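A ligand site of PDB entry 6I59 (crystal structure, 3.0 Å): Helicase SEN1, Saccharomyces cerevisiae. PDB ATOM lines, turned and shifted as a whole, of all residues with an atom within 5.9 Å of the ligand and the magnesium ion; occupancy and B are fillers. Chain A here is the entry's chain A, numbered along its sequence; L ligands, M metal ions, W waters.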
ATOM      1  N   LYS A 243      16.554  -6.695 -16.000  1.00  0.00           N
ATOM      2  CA  LYS A 243      15.171  -6.317 -16.288  1.00  0.00           C
ATOM      3  C   LYS A 243      14.715  -6.916 -17.627  1.00  0.00           C
ATOM      4  O   LYS A 243      14.285  -6.222 -18.541  1.00  0.00           O
ATOM      5  CB  LYS A 243      15.011  -4.784 -16.292  1.00  0.00           C
ATOM      6  CG  LYS A 243      15.428  -4.122 -14.989  1.00  0.00           C
ATOM      7  CD  LYS A 243      14.929  -2.695 -14.929  1.00  0.00           C
ATOM      8  CE  LYS A 243      15.384  -1.994 -13.655  1.00  0.00           C
ATOM      9  NZ  LYS A 243      16.858  -1.852 -13.606  1.00  0.00           N
ATOM     10  N   LEU A 244      14.831  -8.236 -17.712  1.00  0.00           N
ATOM     11  CA  LEU A 244      14.512  -8.992 -18.904  1.00  0.00           C
ATOM     12  C   LEU A 244      13.374  -9.951 -18.601  1.00  0.00           C
ATOM     13  O   LEU A 244      12.984 -10.133 -17.448  1.00  0.00           O
ATOM     14  CB  LEU A 244      15.724  -9.775 -19.411  1.00  0.00           C
ATOM     15  CG  LEU A 244      17.022  -8.994 -19.627  1.00  0.00           C
ATOM     16  CD1 LEU A 244      18.176  -9.963 -19.798  1.00  0.00           C
ATOM     17  CD2 LEU A 244      16.915  -8.069 -20.823  1.00  0.00           C
ATOM     18  N   ASN A 245      12.851 -10.573 -19.650  1.00  0.00           N
ATOM     19  CA  ASN A 245      11.917 -11.669 -19.454  1.00  0.00           C
ATOM     20  C   ASN A 245      12.668 -12.989 -19.413  1.00  0.00           C
ATOM     21  O   ASN A 245      13.886 -13.064 -19.637  1.00  0.00           O
ATOM     22  CB  ASN A 245      10.840 -11.679 -20.548  1.00  0.00           C
ATOM     23  CG  ASN A 245      11.404 -11.826 -21.941  1.00  0.00           C
ATOM     24  OD1 ASN A 245      12.187 -12.733 -22.228  1.00  0.00           O
ATOM     25  ND2 ASN A 245      11.002 -10.917 -22.822  1.00  0.00           N
ATOM     26  N   GLN A 248      14.639 -14.152 -22.641  1.00  0.00           N
ATOM     27  CA  GLN A 248      15.868 -13.391 -22.826  1.00  0.00           C
ATOM     28  C   GLN A 248      16.935 -13.812 -21.825  1.00  0.00           C
ATOM     29  O   GLN A 248      18.089 -14.044 -22.195  1.00  0.00           O
ATOM     30  CB  GLN A 248      15.563 -11.898 -22.726  1.00  0.00           C
ATOM     31  CG  GLN A 248      14.582 -11.394 -23.777  1.00  0.00           C
ATOM     32  CD  GLN A 248      14.051 -10.009 -23.457  1.00  0.00           C
ATOM     33  OE1 GLN A 248      14.051  -9.584 -22.304  1.00  0.00           O
ATOM     34  NE2 GLN A 248      13.585  -9.294 -24.477  1.00  0.00           N
ATOM     35  N   GLY A 266      14.754 -14.045 -32.572  1.00  0.00           N
ATOM     36  CA  GLY A 266      13.864 -13.022 -32.083  1.00  0.00           C
ATOM     37  C   GLY A 266      12.879 -12.563 -33.127  1.00  0.00           C
ATOM     38  O   GLY A 266      13.242 -11.888 -34.103  1.00  0.00           O
ATOM     39  N   PRO A 267      11.610 -12.923 -32.960  1.00  0.00           N
ATOM     40  CA  PRO A 267      10.552 -12.380 -33.824  1.00  0.00           C
ATOM     41  C   PRO A 267      10.502 -10.867 -33.715  1.00  0.00           C
ATOM     42  O   PRO A 267      11.185 -10.275 -32.860  1.00  0.00           O
ATOM     43  CB  PRO A 267       9.278 -13.023 -33.260  1.00  0.00           C
ATOM     44  CG  PRO A 267       9.745 -14.288 -32.616  1.00  0.00           C
ATOM     45  CD  PRO A 267      11.120 -13.983 -32.061  1.00  0.00           C
ATOM     46  N   PRO A 268       9.729 -10.193 -34.573  1.00  0.00           N
ATOM     47  CA  PRO A 268       9.680  -8.722 -34.521  1.00  0.00           C
ATOM     48  C   PRO A 268       9.305  -8.208 -33.133  1.00  0.00           C
ATOM     49  O   PRO A 268       8.289  -8.611 -32.547  1.00  0.00           O
ATOM     50  CB  PRO A 268       8.598  -8.372 -35.546  1.00  0.00           C
ATOM     51  CG  PRO A 268       8.668  -9.469 -36.524  1.00  0.00           C
ATOM     52  CD  PRO A 268       8.973 -10.709 -35.736  1.00  0.00           C
ATOM     53  N   GLY A 269      10.138  -7.323 -32.606  1.00  0.00           N
ATOM     54  CA  GLY A 269       9.827  -6.620 -31.381  1.00  0.00           C
ATOM     55  C   GLY A 269      10.014  -7.425 -30.114  1.00  0.00           C
ATOM     56  O   GLY A 269       9.366  -7.131 -29.103  1.00  0.00           O
ATOM     57  N   THR A 270      10.885  -8.424 -30.134  1.00  0.00           N
ATOM     58  CA  THR A 270      11.074  -9.301 -28.988  1.00  0.00           C
ATOM     59  C   THR A 270      12.338  -8.998 -28.195  1.00  0.00           C
ATOM     60  O   THR A 270      12.615  -9.688 -27.215  1.00  0.00           O
ATOM     61  CB  THR A 270      11.076 -10.761 -29.444  1.00  0.00           C
ATOM     62  OG1 THR A 270      12.093 -10.967 -30.420  1.00  0.00           O
ATOM     63  CG2 THR A 270       9.720 -11.131 -30.052  1.00  0.00           C
ATOM     64  N   GLY A 271      13.108  -7.994 -28.598  1.00  0.00           N
ATOM     65  CA  GLY A 271      14.262  -7.575 -27.824  1.00  0.00           C
ATOM     66  C   GLY A 271      15.577  -8.223 -28.192  1.00  0.00           C
ATOM     67  O   GLY A 271      16.362  -8.590 -27.312  1.00  0.00           O
ATOM     68  N   LYS A 272      15.860  -8.348 -29.498  1.00  0.00           N
ATOM     69  CA  LYS A 272      17.143  -8.888 -29.923  1.00  0.00           C
ATOM     70  C   LYS A 272      18.291  -8.001 -29.455  1.00  0.00           C
ATOM     71  O   LYS A 272      19.241  -8.457 -28.811  1.00  0.00           O
ATOM     72  CB  LYS A 272      17.161  -9.041 -31.448  1.00  0.00           C
ATOM     73  CG  LYS A 272      16.224 -10.109 -31.985  1.00  0.00           C
ATOM     74  CD  LYS A 272      16.191 -10.138 -33.498  1.00  0.00           C
ATOM     75  CE  LYS A 272      15.488  -8.911 -34.082  1.00  0.00           C
ATOM     76  NZ  LYS A 272      14.032  -8.878 -33.764  1.00  0.00           N
ATOM     77  N   THR A 273      18.188  -6.700 -29.734  1.00  0.00           N
ATOM     78  CA  THR A 273      19.272  -5.786 -29.378  1.00  0.00           C
ATOM     79  C   THR A 273      19.378  -5.625 -27.861  1.00  0.00           C
ATOM     80  O   THR A 273      20.495  -5.586 -27.313  1.00  0.00           O
ATOM     81  CB  THR A 273      19.066  -4.449 -30.092  1.00  0.00           C
ATOM     82  OG1 THR A 273      18.893  -4.697 -31.499  1.00  0.00           O
ATOM     83  CG2 THR A 273      20.266  -3.543 -29.895  1.00  0.00           C
ATOM     84  N   LYS A 274      18.244  -5.546 -27.148  1.00  0.00           N
ATOM     85  CA  LYS A 274      18.274  -5.485 -25.693  1.00  0.00           C
ATOM     86  C   LYS A 274      18.962  -6.705 -25.097  1.00  0.00           C
ATOM     87  O   LYS A 274      19.774  -6.599 -24.166  1.00  0.00           O
ATOM     88  CB  LYS A 274      16.844  -5.348 -25.155  1.00  0.00           C
ATOM     89  CG  LYS A 274      16.732  -5.242 -23.647  1.00  0.00           C
ATOM     90  CD  LYS A 274      15.346  -4.787 -23.276  1.00  0.00           C
ATOM     91  CE  LYS A 274      15.362  -3.795 -22.110  1.00  0.00           C
ATOM     92  NZ  LYS A 274      14.237  -2.830 -22.207  1.00  0.00           N
ATOM     93  N   THR A 275      18.664  -7.891 -25.650  1.00  0.00           N
ATOM     94  CA  THR A 275      19.319  -9.111 -25.196  1.00  0.00           C
ATOM     95  C   THR A 275      20.819  -9.068 -25.493  1.00  0.00           C
ATOM     96  O   THR A 275      21.615  -9.595 -24.718  1.00  0.00           O
ATOM     97  CB  THR A 275      18.666 -10.316 -25.862  1.00  0.00           C
ATOM     98  OG1 THR A 275      17.273 -10.348 -25.510  1.00  0.00           O
ATOM     99  CG2 THR A 275      19.323 -11.618 -25.421  1.00  0.00           C
ATOM    100  N   GLU A 327      22.900   1.621 -34.023  1.00  0.00           N
ATOM    101  CA  GLU A 327      21.902   1.466 -32.962  1.00  0.00           C
ATOM    102  C   GLU A 327      22.509   0.775 -31.752  1.00  0.00           C
ATOM    103  O   GLU A 327      22.266   1.174 -30.606  1.00  0.00           O
ATOM    104  CB  GLU A 327      20.676   0.700 -33.466  1.00  0.00           C
ATOM    105  CG  GLU A 327      19.593   0.597 -32.406  1.00  0.00           C
ATOM    106  CD  GLU A 327      18.379  -0.167 -32.879  1.00  0.00           C
ATOM    107  OE1 GLU A 327      18.306  -0.471 -34.096  1.00  0.00           O
ATOM    108  OE2 GLU A 327      17.502  -0.479 -32.047  1.00  0.00           O
ATOM    109  N   ARG A 331      22.713   2.633 -28.047  1.00  0.00           N
ATOM    110  CA  ARG A 331      22.112   2.025 -26.878  1.00  0.00           C
ATOM    111  C   ARG A 331      23.154   1.582 -25.859  1.00  0.00           C
ATOM    112  O   ARG A 331      22.823   1.420 -24.681  1.00  0.00           O
ATOM    113  CB  ARG A 331      21.225   0.856 -27.290  1.00  0.00           C
ATOM    114  CG  ARG A 331      19.999   1.317 -28.069  1.00  0.00           C
ATOM    115  CD  ARG A 331      19.249   0.184 -28.745  1.00  0.00           C
ATOM    116  NE  ARG A 331      18.561  -0.679 -27.789  1.00  0.00           N
ATOM    117  CZ  ARG A 331      17.652  -1.582 -28.143  1.00  0.00           C
ATOM    118  NH1 ARG A 331      17.315  -1.744 -29.414  1.00  0.00           N
ATOM    119  NH2 ARG A 331      17.067  -2.341 -27.213  1.00  0.00           N
ATOM    120  N   ASP A 435      24.382  -9.157 -34.380  1.00  0.00           N
ATOM    121  CA  ASP A 435      22.995  -8.750 -34.454  1.00  0.00           C
ATOM    122  C   ASP A 435      22.519  -8.809 -35.908  1.00  0.00           C
ATOM    123  O   ASP A 435      23.315  -8.778 -36.846  1.00  0.00           O
ATOM    124  CB  ASP A 435      22.810  -7.328 -33.908  1.00  0.00           C
ATOM    125  CG  ASP A 435      21.414  -7.071 -33.373  1.00  0.00           C
ATOM    126  OD1 ASP A 435      20.563  -7.974 -33.486  1.00  0.00           O
ATOM    127  OD2 ASP A 435      21.170  -5.975 -32.842  1.00  0.00           O
ATOM    128  N   GLU A 436      21.192  -8.912 -36.076  1.00  0.00           N
ATOM    129  CA  GLU A 436      20.572  -8.989 -37.404  1.00  0.00           C
ATOM    130  C   GLU A 436      21.222 -10.090 -38.237  1.00  0.00           C
ATOM    131  O   GLU A 436      21.452  -9.946 -39.440  1.00  0.00           O
ATOM    132  CB  GLU A 436      20.670  -7.638 -38.115  1.00  0.00           C
ATOM    133  CG  GLU A 436      20.190  -6.477 -37.267  1.00  0.00           C
ATOM    134  CD  GLU A 436      18.688  -6.338 -37.259  1.00  0.00           C
ATOM    135  OE1 GLU A 436      18.157  -5.687 -38.183  1.00  0.00           O
ATOM    136  OE2 GLU A 436      18.024  -6.893 -36.352  1.00  0.00           O
ATOM    137  N   LEU A 496      13.070 -15.802 -28.217  1.00  0.00           N
ATOM    138  CA  LEU A 496      12.557 -14.686 -27.432  1.00  0.00           C
ATOM    139  C   LEU A 496      11.071 -14.584 -27.737  1.00  0.00           C
ATOM    140  O   LEU A 496      10.695 -14.369 -28.888  1.00  0.00           O
ATOM    141  CB  LEU A 496      13.288 -13.392 -27.780  1.00  0.00           C
ATOM    142  CG  LEU A 496      14.814 -13.470 -27.849  1.00  0.00           C
ATOM    143  CD1 LEU A 496      15.380 -12.104 -28.155  1.00  0.00           C
ATOM    144  CD2 LEU A 496      15.399 -14.025 -26.565  1.00  0.00           C
ATOM    145  N   VAL A 498       8.267 -12.807 -26.281  1.00  0.00           N
ATOM    146  CA  VAL A 498       7.353 -11.734 -25.904  1.00  0.00           C
ATOM    147  C   VAL A 498       7.626 -10.552 -26.820  1.00  0.00           C
ATOM    148  O   VAL A 498       8.749 -10.035 -26.842  1.00  0.00           O
ATOM    149  CB  VAL A 498       7.504 -11.302 -24.438  1.00  0.00           C
ATOM    150  CG1 VAL A 498       6.385 -10.352 -24.060  1.00  0.00           C
ATOM    151  CG2 VAL A 498       7.540 -12.498 -23.511  1.00  0.00           C
ATOM    152  N   TYR A 500       6.823  -6.580 -28.024  1.00  0.00           N
ATOM    153  CA  TYR A 500       6.483  -5.333 -27.368  1.00  0.00           C
ATOM    154  C   TYR A 500       6.144  -4.238 -28.376  1.00  0.00           C
ATOM    155  O   TYR A 500       6.397  -3.053 -28.132  1.00  0.00           O
ATOM    156  CB  TYR A 500       7.609  -4.865 -26.456  1.00  0.00           C
ATOM    157  CG  TYR A 500       8.008  -5.861 -25.388  1.00  0.00           C
ATOM    158  CD1 TYR A 500       7.425  -5.820 -24.119  1.00  0.00           C
ATOM    159  CD2 TYR A 500       8.980  -6.830 -25.626  1.00  0.00           C
ATOM    160  CE1 TYR A 500       7.781  -6.734 -23.138  1.00  0.00           C
ATOM    161  CE2 TYR A 500       9.331  -7.740 -24.653  1.00  0.00           C
ATOM    162  CZ  TYR A 500       8.739  -7.680 -23.408  1.00  0.00           C
ATOM    163  OH  TYR A 500       9.108  -8.589 -22.432  1.00  0.00           O
ATOM    164  N   ARG A 501       5.556  -4.613 -29.510  1.00  0.00           N
ATOM    165  CA  ARG A 501       5.244  -3.681 -30.584  1.00  0.00           C
ATOM    166  C   ARG A 501       3.770  -3.608 -30.907  1.00  0.00           C
ATOM    167  O   ARG A 501       3.199  -2.511 -30.994  1.00  0.00           O
ATOM    168  CB  ARG A 501       6.003  -4.064 -31.862  1.00  0.00           C
ATOM    169  CG  ARG A 501       7.470  -3.723 -31.880  1.00  0.00           C
ATOM    170  CD  ARG A 501       8.133  -4.209 -33.174  1.00  0.00           C
ATOM    171  NE  ARG A 501       7.556  -3.619 -34.386  1.00  0.00           N
ATOM    172  CZ  ARG A 501       6.724  -4.252 -35.209  1.00  0.00           C
ATOM    173  NH1 ARG A 501       6.247  -3.642 -36.295  1.00  0.00           N
ATOM    174  NH2 ARG A 501       6.351  -5.497 -34.949  1.00  0.00           N
HETATM  175  P1  LIG L   1      14.605  -5.960 -31.509  1.00  0.00           P
HETATM  176  O1  LIG L   1      16.089  -5.689 -31.395  1.00  0.00           O
HETATM  177  O2  LIG L   1      13.903  -5.166 -32.579  1.00  0.00           O
HETATM  178  O3  LIG L   1      14.263  -7.436 -31.472  1.00  0.00           O
HETATM  179  P2  LIG L   1      14.620  -4.085 -29.417  1.00  0.00           P
HETATM  180  O4  LIG L   1      14.952  -3.032 -30.451  1.00  0.00           O
HETATM  181  O5  LIG L   1      15.697  -4.577 -28.478  1.00  0.00           O
HETATM  182  O6  LIG L   1      13.988  -5.367 -30.143  1.00  0.00           O
HETATM  183  O7  LIG L   1      13.390  -3.550 -28.553  1.00  0.00           O
HETATM  184  C1  LIG L   1      12.048  -3.635 -29.039  1.00  0.00           C
HETATM  185  C2  LIG L   1      11.139  -2.996 -28.004  1.00  0.00           C
HETATM  186  O8  LIG L   1      10.755  -3.975 -27.030  1.00  0.00           O
HETATM  187  C3  LIG L   1      11.828  -1.882 -27.238  1.00  0.00           C
HETATM  188  O9  LIG L   1      10.964  -0.750 -27.175  1.00  0.00           O
HETATM  189  C4  LIG L   1      12.057  -2.420 -25.837  1.00  0.00           C
HETATM  190  O10 LIG L   1      11.912  -1.380 -24.879  1.00  0.00           O
HETATM  191  C5  LIG L   1      10.981  -3.480 -25.716  1.00  0.00           C
HETATM  192  N1  LIG L   1      11.407  -4.592 -24.830  1.00  0.00           N
HETATM  193  C6  LIG L   1      12.216  -5.617 -25.161  1.00  0.00           C
HETATM  194  N2  LIG L   1      12.398  -6.455 -24.118  1.00  0.00           N
HETATM  195  C7  LIG L   1      11.697  -5.967 -23.074  1.00  0.00           C
HETATM  196  C8  LIG L   1      11.433  -6.346 -21.660  1.00  0.00           C
HETATM  197  N3  LIG L   1      11.973  -7.449 -21.098  1.00  0.00           N
HETATM  198  N4  LIG L   1      10.633  -5.542 -20.938  1.00  0.00           N
HETATM  199  C9  LIG L   1      10.083  -4.427 -21.452  1.00  0.00           C
HETATM  200  N5  LIG L   1      10.268  -4.025 -22.722  1.00  0.00           N
HETATM  201  C10 LIG L   1      11.047  -4.734 -23.563  1.00  0.00           C
HETATM  202 MG    MG M   1      17.368  -4.765 -32.929  1.00  0.00          MG
HETATM  203  O   HOH W   1      11.641  -3.499 -32.636  1.00  0.00           O
HETATM  204  O   HOH W   2       8.763  -0.628 -28.970  1.00  0.00           O
HETATM  205  O   HOH W   3       8.920  -1.913 -23.160  1.00  0.00           O
HETATM  206  O   HOH W   4      18.035  -6.708 -33.795  1.00  0.00           O
HETATM  207  O   HOH W   5      18.481  -3.534 -34.164  1.00  0.00           O
HETATM  208  O   HOH W   6      15.900  -4.751 -34.342  1.00  0.00           O
HETATM  209  O   HOH W   7      10.608  -1.573 -31.252  1.00  0.00           O
HETATM  210  O   HOH W   8      16.632  -2.955 -32.196  1.00  0.00           O
HETATM  211  O   HOH W   9      10.123   0.307 -24.021  1.00  0.00           O
HETATM  212  O   HOH W  10      12.291   1.565 -26.795  1.00  0.00           O
HETATM  213  O   HOH W  11      14.079  -0.404 -30.135  1.00  0.00           O
HETATM  214  O   HOH W  12      12.357  -6.516 -34.233  1.00  0.00           O
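Water W4 lies within hydrogen-bond range of the side-chain carboxylate (OE2) of Glu 436 (2.6 Å) and the side-chain carboxylate (OD1) of Asp 435 (2.8 Å). Water W8 lies within hydrogen-bond range of an oxygen (O4) of the ligand (2.4 Å), the side-chain carboxylate of Glu 327 (2.6 Å) and the guanidinium group of Arg 331 (3.1 Å). Water W12 lies within hydrogen-bond range of an oxygen (O2) of the ligand (2.6 Å), the backbone NH (N) of Gly 269 (2.9 Å) and the side-chain amino group (NZ) of Lys 272 (2.9 Å). Water W2 bridges O9 of the ligand (2.8 Å) and O of Tyr 500 (3.5 Å).
Merely in contact with the magnesium ion: Asp 435 (3.99 Å). Two residues have an atom within 4 Å of the magnesium ion: Thr 273 and Asp 435.
Water W6 binds the magnesium ion (2.0 Å). The magnesium ion is bound by water W5 (2.1 Å). The magnesium ion is bound by water W8. The magnesium ion is bound by the side-chain hydroxyl (OG1) of Thr 273 (2.1 Å). The magnesium ion is bound by an oxygen (O1) of the ligand (2.2 Å). The magnesium ion is bound by water W4, at 2.2 Å.
O of Gly 271 is in hydrogen-bond range of OG1 of Thr 275, at 2.7 Å. The side-chain amide nitrogen (NE2) of Gln 248 lies within hydrogen-bond range of the backbone carbonyl oxygen (O) of Thr 270. The backbone carbonyl oxygen (O) of Gly 269 sits at hydrogen-bond distance from the backbone NH (N) of Tyr 500, 2.8 Å away. The side-chain amino group of Lys 272 is in hydrogen-bond range of the backbone carbonyl oxygen of Pro 267. The backbone carbonyl oxygen of Gly 266 is in hydrogen-bond range of the side-chain amino group of Lys 272 (3.1 Å). OG1 of Thr 273 sits close to OD2 of Asp 435. OH of Tyr 500 is in hydrogen-bond range of ND2 of Asn 245. The backbone NH of Gln 248 is in hydrogen-bond range of the side-chain amide oxygen of Asn 245 (2.9 Å).
Merely in contact with the ligand: Lys 243 (3.7 Å), Leu 244 (3.7 Å), Asn 245 (3.6 Å), Thr 270 (3.8 Å) and Glu 327 (3.9 Å). Within 4 Å of the ligand: Lys 243, Leu 244, Asn 245, Gln 248, Thr 270, Gly 271, Lys 272, Thr 273, Lys 274, Glu 327, Arg 331 and Tyr 500. Along chain A the residues within 4 Å of the ligand span positions 243 to 500. The nearest printed residue that does not touch the ligand is Gly 269 (4.02 Å).
N of Lys 272 sits at hydrogen-bond distance from O3 of the ligand. The guanidinium group (NH1) of Arg 331 is in salt-bridge range of an oxygen (O4) of the ligand (2.9 Å). The backbone NH of Lys 274 sits at hydrogen-bond distance from an oxygen (O5) of the ligand (3.0 Å). An oxygen (O1) of the ligand sits close to the backbone NH of Thr 273. OH of Tyr 500 sits close to N3 of the ligand (3.4 Å). The backbone NH (N) of Gly 271 lies within hydrogen-bond range of an oxygen (O3) of the ligand (3.1 Å). A nitrogen (N2) of the ligand is in hydrogen-bond range of the side-chain amide nitrogen (NE2) of Gln 248, at 3.1 Å. An oxygen (O3) of the ligand lies within salt-bridge range of the side-chain amino group (NZ) of Lys 272 (2.7 Å).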
